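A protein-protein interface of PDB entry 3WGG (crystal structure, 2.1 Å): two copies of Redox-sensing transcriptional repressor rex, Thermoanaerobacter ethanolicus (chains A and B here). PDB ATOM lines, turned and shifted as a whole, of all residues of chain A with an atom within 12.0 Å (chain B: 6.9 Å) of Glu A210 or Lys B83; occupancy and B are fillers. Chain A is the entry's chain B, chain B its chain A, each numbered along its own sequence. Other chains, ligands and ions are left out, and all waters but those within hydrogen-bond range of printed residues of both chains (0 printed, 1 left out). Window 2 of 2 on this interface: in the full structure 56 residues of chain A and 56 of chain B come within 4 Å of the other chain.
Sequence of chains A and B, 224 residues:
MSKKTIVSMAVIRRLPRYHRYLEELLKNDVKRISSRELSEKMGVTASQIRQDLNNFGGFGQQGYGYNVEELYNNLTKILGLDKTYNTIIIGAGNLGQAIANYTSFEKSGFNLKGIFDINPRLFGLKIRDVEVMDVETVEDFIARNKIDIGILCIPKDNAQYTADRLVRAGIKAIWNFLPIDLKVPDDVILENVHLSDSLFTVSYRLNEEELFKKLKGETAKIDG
Phe B110 touches Leu A199. Phe A200 touches Leu B81 (CD2 to CD1, 3.6 Å). Phe A200 touches Ser B108. Phe B110 touches Phe A200 (CE1 to CE1, 3.5 Å). Ser A203 touches Leu B81. Tyr B85 touches Ser A203 (OH to CB, 3.7 Å). Tyr B85 touches Leu A206 (CD1 to CD1, 3.7 Å). ND2 of Asn A207 touches CA of Gly B80, 3.6 Å away. Lys B83 touches Asn A207. CD2 of Phe A212 touches CD1 of Ile B6 (3.7 Å).
No position is printed for both chains. Of the 13 pairs that touch across the chains among the printed residues, none has its exchanged pair printed and touching as well.
Hydrophobic or aromatic side chains of chain B within 4 Å of the printed part of chain A: Ile B6, Leu B81, Tyr B85 and Phe B110. Of the 17 printed residues of chain A, 8 touch a printed residue of chain B. Hydrophobic or aromatic side chains of chain A that line the printed part of chain B: Leu A199, Phe A200, Leu A206 and Phe A212.
Printed residues of chain B within 4 Å of Phe A200: Leu B81, Ser B108 and Phe B110. Printed residues of chain B within 4 Å of Asn A207: Gly B80 and Lys B83. Glu A209 touches none of the printed residues of chain B. Glu A210 touches one residue of chain B. Lys A213 touches none of the printed residues of chain B. Printed residues of chain A within 4 Å of Ile B6: Glu A208 (2.8 Å) and Phe A212 (3.7 Å). Of the printed residues of chain A, Leu B81 touches Phe A200 and Ser A203. No residue of chain A comes within 4 Å of Asp B82. Printed residues of chain A within 4 Å of Lys B83: Asn A207 and Glu A210. No residue of chain A comes within 4 Å of Thr B84. Of chain A, only Ser A203 (3.7 Å) and Leu A206 (3.7 Å) come within 4 Å of Tyr B85. Printed residues of chain A within 4 Å of Ser B108: Phe A200 (3.6 Å). The nearest residue of chain B that does not touch Glu A210 is Ile B6 (6.7 Å).
The backbone NH (N) of Tyr B85 lies within hydrogen-bond range of the backbone carbonyl oxygen (O) of Gly B109, at 2.9 Å. OH of Tyr A204 sits at hydrogen-bond distance from OE2 of Glu A208 (2.6 Å). N of Leu B81 lies within hydrogen-bond range of O of Thr B76 (2.8 Å). O of Phe A200 is in hydrogen-bond range of OG of Ser A203 (2.9 Å). The side-chain hydroxyl (OH) of Tyr B85 is in hydrogen-bond range of the backbone carbonyl oxygen (O) of Gly B80, 2.6 Å away.
OE1 of Glu A210 is in salt-bridge range of NZ of Lys B83, 3.8 Å away. OE1 of Glu A208 lies within hydrogen-bond range of N of Ile B6, at 2.8 Å.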
ATOM      1  N   LEU A 199       3.380 -18.520  18.701  1.00  0.00           N
ATOM      2  CA  LEU A 199       4.331 -17.415  18.576  1.00  0.00           C
ATOM      3  C   LEU A 199       3.976 -16.156  19.397  1.00  0.00           C
ATOM      4  O   LEU A 199       4.838 -15.515  19.991  1.00  0.00           O
ATOM      5  CB  LEU A 199       4.481 -17.028  17.108  1.00  0.00           C
ATOM      6  CG  LEU A 199       5.383 -15.805  16.881  1.00  0.00           C
ATOM      7  CD1 LEU A 199       6.802 -16.023  17.483  1.00  0.00           C
ATOM      8  CD2 LEU A 199       5.441 -15.479  15.398  1.00  0.00           C
ATOM      9  N   PHE A 200       2.698 -15.790  19.383  1.00  0.00           N
ATOM     10  CA  PHE A 200       2.207 -14.612  20.071  1.00  0.00           C
ATOM     11  C   PHE A 200       2.297 -14.733  21.582  1.00  0.00           C
ATOM     12  O   PHE A 200       2.270 -13.718  22.282  1.00  0.00           O
ATOM     13  CB  PHE A 200       0.764 -14.240  19.614  1.00  0.00           C
ATOM     14  CG  PHE A 200       0.694 -13.748  18.171  1.00  0.00           C
ATOM     15  CD1 PHE A 200       1.850 -13.683  17.382  1.00  0.00           C
ATOM     16  CD2 PHE A 200      -0.535 -13.409  17.581  1.00  0.00           C
ATOM     17  CE1 PHE A 200       1.773 -13.278  16.002  1.00  0.00           C
ATOM     18  CE2 PHE A 200      -0.604 -13.011  16.209  1.00  0.00           C
ATOM     19  CZ  PHE A 200       0.531 -12.900  15.439  1.00  0.00           C
ATOM     20  N   VAL A 202       5.023 -15.629  22.700  1.00  0.00           N
ATOM     21  CA  VAL A 202       6.442 -15.381  22.922  1.00  0.00           C
ATOM     22  C   VAL A 202       6.576 -13.878  23.051  1.00  0.00           C
ATOM     23  O   VAL A 202       7.194 -13.376  24.000  1.00  0.00           O
ATOM     24  CB  VAL A 202       7.301 -15.896  21.745  1.00  0.00           C
ATOM     25  CG1 VAL A 202       8.670 -15.221  21.747  1.00  0.00           C
ATOM     26  CG2 VAL A 202       7.410 -17.411  21.808  1.00  0.00           C
ATOM     27  N   SER A 203       5.976 -13.173  22.093  1.00  0.00           N
ATOM     28  CA  SER A 203       5.856 -11.732  22.192  1.00  0.00           C
ATOM     29  C   SER A 203       5.138 -11.301  23.496  1.00  0.00           C
ATOM     30  O   SER A 203       5.555 -10.362  24.149  1.00  0.00           O
ATOM     31  CB  SER A 203       5.150 -11.175  20.971  1.00  0.00           C
ATOM     32  OG  SER A 203       3.955 -11.905  20.738  1.00  0.00           O
ATOM     33  N   TYR A 204       4.097 -12.010  23.901  1.00  0.00           N
ATOM     34  CA  TYR A 204       3.426 -11.618  25.142  1.00  0.00           C
ATOM     35  C   TYR A 204       4.446 -11.653  26.259  1.00  0.00           C
ATOM     36  O   TYR A 204       4.536 -10.724  27.097  1.00  0.00           O
ATOM     37  CB  TYR A 204       2.293 -12.597  25.498  1.00  0.00           C
ATOM     38  CG  TYR A 204       1.753 -12.299  26.864  1.00  0.00           C
ATOM     39  CD1 TYR A 204       0.692 -11.422  27.032  1.00  0.00           C
ATOM     40  CD2 TYR A 204       2.371 -12.833  28.011  1.00  0.00           C
ATOM     41  CE1 TYR A 204       0.212 -11.099  28.352  1.00  0.00           C
ATOM     42  CE2 TYR A 204       1.921 -12.521  29.318  1.00  0.00           C
ATOM     43  CZ  TYR A 204       0.849 -11.639  29.478  1.00  0.00           C
ATOM     44  OH  TYR A 204       0.423 -11.334  30.762  1.00  0.00           O
ATOM     45  N   ARG A 205       5.178 -12.763  26.329  1.00  0.00           N
ATOM     46  CA  ARG A 205       6.092 -12.922  27.466  1.00  0.00           C
ATOM     47  C   ARG A 205       7.279 -12.003  27.471  1.00  0.00           C
ATOM     48  O   ARG A 205       7.692 -11.566  28.518  1.00  0.00           O
ATOM     49  CB  ARG A 205       6.522 -14.360  27.677  1.00  0.00           C
ATOM     50  CG  ARG A 205       5.454 -15.203  28.281  1.00  0.00           C
ATOM     51  CD  ARG A 205       5.959 -16.600  28.278  1.00  0.00           C
ATOM     52  NE  ARG A 205       5.583 -17.255  27.020  1.00  0.00           N
ATOM     53  CZ  ARG A 205       5.891 -18.528  26.722  1.00  0.00           C
ATOM     54  NH1 ARG A 205       6.614 -19.243  27.587  1.00  0.00           N
ATOM     55  NH2 ARG A 205       5.474 -19.089  25.583  1.00  0.00           N
ATOM     56  N   LEU A 206       7.812 -11.690  26.303  1.00  0.00           N
ATOM     57  CA  LEU A 206       8.908 -10.740  26.193  1.00  0.00           C
ATOM     58  C   LEU A 206       8.482  -9.369  26.715  1.00  0.00           C
ATOM     59  O   LEU A 206       9.297  -8.487  26.985  1.00  0.00           O
ATOM     60  CB  LEU A 206       9.355 -10.621  24.743  1.00  0.00           C
ATOM     61  CG  LEU A 206      10.188 -11.753  24.134  1.00  0.00           C
ATOM     62  CD1 LEU A 206      10.340 -11.546  22.603  1.00  0.00           C
ATOM     63  CD2 LEU A 206      11.588 -11.851  24.828  1.00  0.00           C
ATOM     64  N   ASN A 207       7.183  -9.184  26.867  1.00  0.00           N
ATOM     65  CA  ASN A 207       6.660  -7.841  27.030  1.00  0.00           C
ATOM     66  C   ASN A 207       5.960  -7.674  28.369  1.00  0.00           C
ATOM     67  O   ASN A 207       5.550  -6.564  28.701  1.00  0.00           O
ATOM     68  CB  ASN A 207       5.684  -7.598  25.874  1.00  0.00           C
ATOM     69  CG  ASN A 207       5.173  -6.182  25.810  1.00  0.00           C
ATOM     70  OD1 ASN A 207       5.935  -5.251  25.512  1.00  0.00           O
ATOM     71  ND2 ASN A 207       3.849  -6.014  25.997  1.00  0.00           N
ATOM     72  N   GLU A 208       5.762  -8.772  29.104  1.00  0.00           N
ATOM     73  CA  GLU A 208       4.810  -8.769  30.204  1.00  0.00           C
ATOM     74  C   GLU A 208       5.253  -7.867  31.370  1.00  0.00           C
ATOM     75  O   GLU A 208       4.404  -7.284  32.046  1.00  0.00           O
ATOM     76  CB  GLU A 208       4.547 -10.160  30.743  1.00  0.00           C
ATOM     77  CG  GLU A 208       3.328 -10.249  31.672  1.00  0.00           C
ATOM     78  CD  GLU A 208       3.275 -11.556  32.451  1.00  0.00           C
ATOM     79  OE1 GLU A 208       4.331 -11.995  32.972  1.00  0.00           O
ATOM     80  OE2 GLU A 208       2.175 -12.146  32.539  1.00  0.00           O
ATOM     81  N   GLU A 209       6.566  -7.841  31.628  1.00  0.00           N
ATOM     82  CA  GLU A 209       7.138  -7.106  32.743  1.00  0.00           C
ATOM     83  C   GLU A 209       6.782  -5.665  32.417  1.00  0.00           C
ATOM     84  O   GLU A 209       6.108  -4.989  33.200  1.00  0.00           O
ATOM     85  CB  GLU A 209       8.660  -7.318  32.786  1.00  0.00           C
ATOM     86  CG  GLU A 209       9.448  -6.317  33.644  1.00  0.00           C
ATOM     87  CD  GLU A 209      10.689  -5.728  32.931  1.00  0.00           C
ATOM     88  OE1 GLU A 209      10.883  -5.980  31.708  1.00  0.00           O
ATOM     89  OE2 GLU A 209      11.448  -4.965  33.588  1.00  0.00           O
ATOM     90  N   GLU A 210       7.148  -5.253  31.203  1.00  0.00           N
ATOM     91  CA  GLU A 210       6.925  -3.903  30.741  1.00  0.00           C
ATOM     92  C   GLU A 210       5.435  -3.527  30.676  1.00  0.00           C
ATOM     93  O   GLU A 210       5.040  -2.443  31.078  1.00  0.00           O
ATOM     94  CB  GLU A 210       7.620  -3.710  29.412  1.00  0.00           C
ATOM     95  CG  GLU A 210       6.916  -2.755  28.504  1.00  0.00           C
ATOM     96  CD  GLU A 210       7.822  -1.649  28.099  1.00  0.00           C
ATOM     97  OE1 GLU A 210       8.219  -1.631  26.907  1.00  0.00           O
ATOM     98  OE2 GLU A 210       8.167  -0.832  28.997  1.00  0.00           O
ATOM     99  N   LEU A 211       4.590  -4.442  30.227  1.00  0.00           N
ATOM    100  CA  LEU A 211       3.165  -4.184  30.216  1.00  0.00           C
ATOM    101  C   LEU A 211       2.719  -3.833  31.616  1.00  0.00           C
ATOM    102  O   LEU A 211       1.830  -3.009  31.798  1.00  0.00           O
ATOM    103  CB  LEU A 211       2.405  -5.424  29.758  1.00  0.00           C
ATOM    104  CG  LEU A 211       0.882  -5.351  29.764  1.00  0.00           C
ATOM    105  CD1 LEU A 211       0.322  -4.397  28.654  1.00  0.00           C
ATOM    106  CD2 LEU A 211       0.344  -6.769  29.605  1.00  0.00           C
ATOM    107  N   PHE A 212       3.308  -4.497  32.603  1.00  0.00           N
ATOM    108  CA  PHE A 212       2.777  -4.422  33.965  1.00  0.00           C
ATOM    109  C   PHE A 212       3.281  -3.256  34.793  1.00  0.00           C
ATOM    110  O   PHE A 212       2.869  -3.083  35.932  1.00  0.00           O
ATOM    111  CB  PHE A 212       2.888  -5.746  34.707  1.00  0.00           C
ATOM    112  CG  PHE A 212       1.677  -6.594  34.546  1.00  0.00           C
ATOM    113  CD1 PHE A 212       0.563  -6.388  35.350  1.00  0.00           C
ATOM    114  CD2 PHE A 212       1.619  -7.572  33.541  1.00  0.00           C
ATOM    115  CE1 PHE A 212      -0.588  -7.173  35.198  1.00  0.00           C
ATOM    116  CE2 PHE A 212       0.477  -8.369  33.388  1.00  0.00           C
ATOM    117  CZ  PHE A 212      -0.632  -8.160  34.207  1.00  0.00           C
ATOM    118  N   LYS A 213       4.157  -2.448  34.205  1.00  0.00           N
ATOM    119  CA  LYS A 213       4.312  -1.057  34.631  1.00  0.00           C
ATOM    120  C   LYS A 213       3.049  -0.321  34.162  1.00  0.00           C
ATOM    121  O   LYS A 213       2.275   0.173  34.993  1.00  0.00           O
ATOM    122  CB  LYS A 213       5.582  -0.438  34.032  1.00  0.00           C
ATOM    123  CG  LYS A 213       6.755  -1.412  33.857  1.00  0.00           C
ATOM    124  CD  LYS A 213       6.990  -2.280  35.100  1.00  0.00           C
ATOM    125  CE  LYS A 213       8.301  -3.090  34.994  1.00  0.00           C
ATOM    126  NZ  LYS A 213       9.028  -3.156  36.299  1.00  0.00           N
ATOM    127  N   LYS A 214       2.831  -0.318  32.836  1.00  0.00           N
ATOM    128  CA  LYS A 214       1.712   0.378  32.162  1.00  0.00           C
ATOM    129  C   LYS A 214       0.360   0.092  32.807  1.00  0.00           C
ATOM    130  O   LYS A 214      -0.206   0.963  33.482  1.00  0.00           O
ATOM    131  CB  LYS A 214       1.675   0.054  30.647  1.00  0.00           C
ATOM    132  CG  LYS A 214       0.353   0.432  29.932  1.00  0.00           C
ATOM    133  CD  LYS A 214       0.560   0.990  28.499  1.00  0.00           C
ATOM    134  CE  LYS A 214      -0.612   1.886  28.038  1.00  0.00           C
ATOM    135  NZ  LYS A 214      -0.743   1.940  26.550  1.00  0.00           N
ATOM    136  N   LEU A 215      -0.152  -1.125  32.603  1.00  0.00           N
ATOM    137  CA  LEU A 215      -1.450  -1.522  33.157  1.00  0.00           C
ATOM    138  C   LEU A 215      -1.488  -1.538  34.699  1.00  0.00           C
ATOM    139  O   LEU A 215      -1.664  -0.477  35.331  1.00  0.00           O
ATOM    140  CB  LEU A 215      -1.940  -2.827  32.510  1.00  0.00           C
ATOM    141  CG  LEU A 215      -2.550  -3.985  33.302  1.00  0.00           C
ATOM    142  CD1 LEU A 215      -4.071  -3.836  33.611  1.00  0.00           C
ATOM    143  CD2 LEU A 215      -2.290  -5.266  32.558  1.00  0.00           C
ATOM    144  N   LYS A 216      -1.266  -2.705  35.307  1.00  0.00           N
ATOM    145  CA  LYS A 216      -1.809  -2.984  36.656  1.00  0.00           C
ATOM    146  C   LYS A 216      -1.303  -2.048  37.765  1.00  0.00           C
ATOM    147  O   LYS A 216      -0.232  -2.254  38.341  1.00  0.00           O
ATOM    148  CB  LYS A 216      -1.617  -4.465  37.004  1.00  0.00           C
ATOM    149  CG  LYS A 216      -2.133  -4.925  38.352  1.00  0.00           C
ATOM    150  CD  LYS A 216      -1.135  -5.922  38.911  1.00  0.00           C
ATOM    151  CE  LYS A 216       0.246  -5.264  39.092  1.00  0.00           C
ATOM    152  NZ  LYS A 216       1.352  -6.258  39.155  1.00  0.00           N
ATOM    153  N   ILE B   6       3.494 -13.294  35.281  1.00  0.00           N
ATOM    154  CA  ILE B   6       2.591 -12.642  36.202  1.00  0.00           C
ATOM    155  C   ILE B   6       1.209 -13.252  36.027  1.00  0.00           C
ATOM    156  O   ILE B   6       0.616 -13.753  36.993  1.00  0.00           O
ATOM    157  CB  ILE B   6       2.545 -11.112  36.008  1.00  0.00           C
ATOM    158  CG1 ILE B   6       3.886 -10.482  36.384  1.00  0.00           C
ATOM    159  CG2 ILE B   6       1.415 -10.518  36.836  1.00  0.00           C
ATOM    160  CD1 ILE B   6       4.171  -9.168  35.696  1.00  0.00           C
ATOM    161  N   THR B  76      -3.899  -6.562  21.042  1.00  0.00           N
ATOM    162  CA  THR B  76      -2.688  -6.414  20.275  1.00  0.00           C
ATOM    163  C   THR B  76      -1.548  -5.916  21.147  1.00  0.00           C
ATOM    164  O   THR B  76      -0.410  -6.413  21.077  1.00  0.00           O
ATOM    165  CB  THR B  76      -2.929  -5.420  19.140  1.00  0.00           C
ATOM    166  OG1 THR B  76      -3.731  -6.073  18.166  1.00  0.00           O
ATOM    167  CG2 THR B  76      -1.624  -5.020  18.515  1.00  0.00           C
ATOM    168  N   GLY B  80       1.997  -7.893  23.063  1.00  0.00           N
ATOM    169  CA  GLY B  80       3.276  -7.254  22.682  1.00  0.00           C
ATOM    170  C   GLY B  80       3.389  -7.023  21.193  1.00  0.00           C
ATOM    171  O   GLY B  80       4.473  -6.758  20.662  1.00  0.00           O
ATOM    172  N   LEU B  81       2.278  -7.126  20.483  1.00  0.00           N
ATOM    173  CA  LEU B  81       2.311  -6.976  19.024  1.00  0.00           C
ATOM    174  C   LEU B  81       2.286  -5.512  18.540  1.00  0.00           C
ATOM    175  O   LEU B  81       2.144  -5.252  17.344  1.00  0.00           O
ATOM    176  CB  LEU B  81       1.160  -7.751  18.360  1.00  0.00           C
ATOM    177  CG  LEU B  81       0.996  -9.256  18.656  1.00  0.00           C
ATOM    178  CD1 LEU B  81      -0.298  -9.832  18.053  1.00  0.00           C
ATOM    179  CD2 LEU B  81       2.231 -10.055  18.173  1.00  0.00           C
ATOM    180  N   ASP B  82       2.390  -4.557  19.446  1.00  0.00           N
ATOM    181  CA  ASP B  82       2.673  -3.188  19.016  1.00  0.00           C
ATOM    182  C   ASP B  82       4.168  -2.921  18.893  1.00  0.00           C
ATOM    183  O   ASP B  82       4.584  -1.758  18.813  1.00  0.00           O
ATOM    184  CB  ASP B  82       2.081  -2.203  20.019  1.00  0.00           C
ATOM    185  CG  ASP B  82       2.517  -2.495  21.477  1.00  0.00           C
ATOM    186  OD1 ASP B  82       2.912  -3.656  21.839  1.00  0.00           O
ATOM    187  OD2 ASP B  82       2.416  -1.532  22.285  1.00  0.00           O
ATOM    188  N   LYS B  83       4.993  -3.962  18.962  1.00  0.00           N
ATOM    189  CA  LYS B  83       6.436  -3.772  18.877  1.00  0.00           C
ATOM    190  C   LYS B  83       6.998  -4.591  17.723  1.00  0.00           C
ATOM    191  O   LYS B  83       6.261  -5.321  17.088  1.00  0.00           O
ATOM    192  CB  LYS B  83       7.101  -4.113  20.213  1.00  0.00           C
ATOM    193  CG  LYS B  83       6.865  -3.015  21.280  1.00  0.00           C
ATOM    194  CD  LYS B  83       7.455  -3.355  22.637  1.00  0.00           C
ATOM    195  CE  LYS B  83       8.980  -3.552  22.556  1.00  0.00           C
ATOM    196  NZ  LYS B  83       9.654  -3.387  23.882  1.00  0.00           N
ATOM    197  N   THR B  84       8.294  -4.438  17.464  1.00  0.00           N
ATOM    198  CA  THR B  84       9.045  -5.178  16.432  1.00  0.00           C
ATOM    199  C   THR B  84      10.008  -6.178  17.048  1.00  0.00           C
ATOM    200  O   THR B  84      10.741  -5.861  17.973  1.00  0.00           O
ATOM    201  CB  THR B  84       9.853  -4.184  15.563  1.00  0.00           C
ATOM    202  OG1 THR B  84       8.921  -3.442  14.768  1.00  0.00           O
ATOM    203  CG2 THR B  84      10.830  -4.925  14.631  1.00  0.00           C
ATOM    204  N   TYR B  85      10.030  -7.388  16.513  1.00  0.00           N
ATOM    205  CA  TYR B  85      10.937  -8.441  16.975  1.00  0.00           C
ATOM    206  C   TYR B  85      11.769  -8.922  15.796  1.00  0.00           C
ATOM    207  O   TYR B  85      11.239  -9.209  14.724  1.00  0.00           O
ATOM    208  CB  TYR B  85      10.131  -9.607  17.528  1.00  0.00           C
ATOM    209  CG  TYR B  85       9.177  -9.167  18.618  1.00  0.00           C
ATOM    210  CD1 TYR B  85       9.589  -9.115  19.952  1.00  0.00           C
ATOM    211  CD2 TYR B  85       7.888  -8.745  18.303  1.00  0.00           C
ATOM    212  CE1 TYR B  85       8.730  -8.677  20.947  1.00  0.00           C
ATOM    213  CE2 TYR B  85       7.055  -8.283  19.260  1.00  0.00           C
ATOM    214  CZ  TYR B  85       7.474  -8.264  20.582  1.00  0.00           C
ATOM    215  OH  TYR B  85       6.635  -7.798  21.535  1.00  0.00           O
ATOM    216  N   SER B 108       2.513  -8.635  11.733  1.00  0.00           N
ATOM    217  CA  SER B 108       2.306  -8.601  13.169  1.00  0.00           C
ATOM    218  C   SER B 108       3.588  -8.180  13.849  1.00  0.00           C
ATOM    219  O   SER B 108       3.639  -8.087  15.064  1.00  0.00           O
ATOM    220  CB  SER B 108       1.768  -9.941  13.709  1.00  0.00           C
ATOM    221  OG  SER B 108       0.931 -10.609  12.746  1.00  0.00           O
ATOM    222  N   GLY B 109       4.637  -7.921  13.078  1.00  0.00           N
ATOM    223  CA  GLY B 109       5.821  -7.298  13.652  1.00  0.00           C
ATOM    224  C   GLY B 109       7.044  -8.184  13.865  1.00  0.00           C
ATOM    225  O   GLY B 109       8.017  -7.762  14.492  1.00  0.00           O
ATOM    226  N   PHE B 110       7.001  -9.410  13.375  1.00  0.00           N
ATOM    227  CA  PHE B 110       8.147 -10.303  13.483  1.00  0.00           C
ATOM    228  C   PHE B 110       8.928 -10.216  12.174  1.00  0.00           C
ATOM    229  O   PHE B 110       8.427 -10.631  11.129  1.00  0.00           O
ATOM    230  CB  PHE B 110       7.670 -11.737  13.756  1.00  0.00           C
ATOM    231  CG  PHE B 110       6.878 -11.851  15.020  1.00  0.00           C
ATOM    232  CD1 PHE B 110       5.524 -11.489  15.042  1.00  0.00           C
ATOM    233  CD2 PHE B 110       7.502 -12.222  16.211  1.00  0.00           C
ATOM    234  CE1 PHE B 110       4.805 -11.519  16.231  1.00  0.00           C
ATOM    235  CE2 PHE B 110       6.787 -12.292  17.376  1.00  0.00           C
ATOM    236  CZ  PHE B 110       5.447 -11.955  17.398  1.00  0.00           C
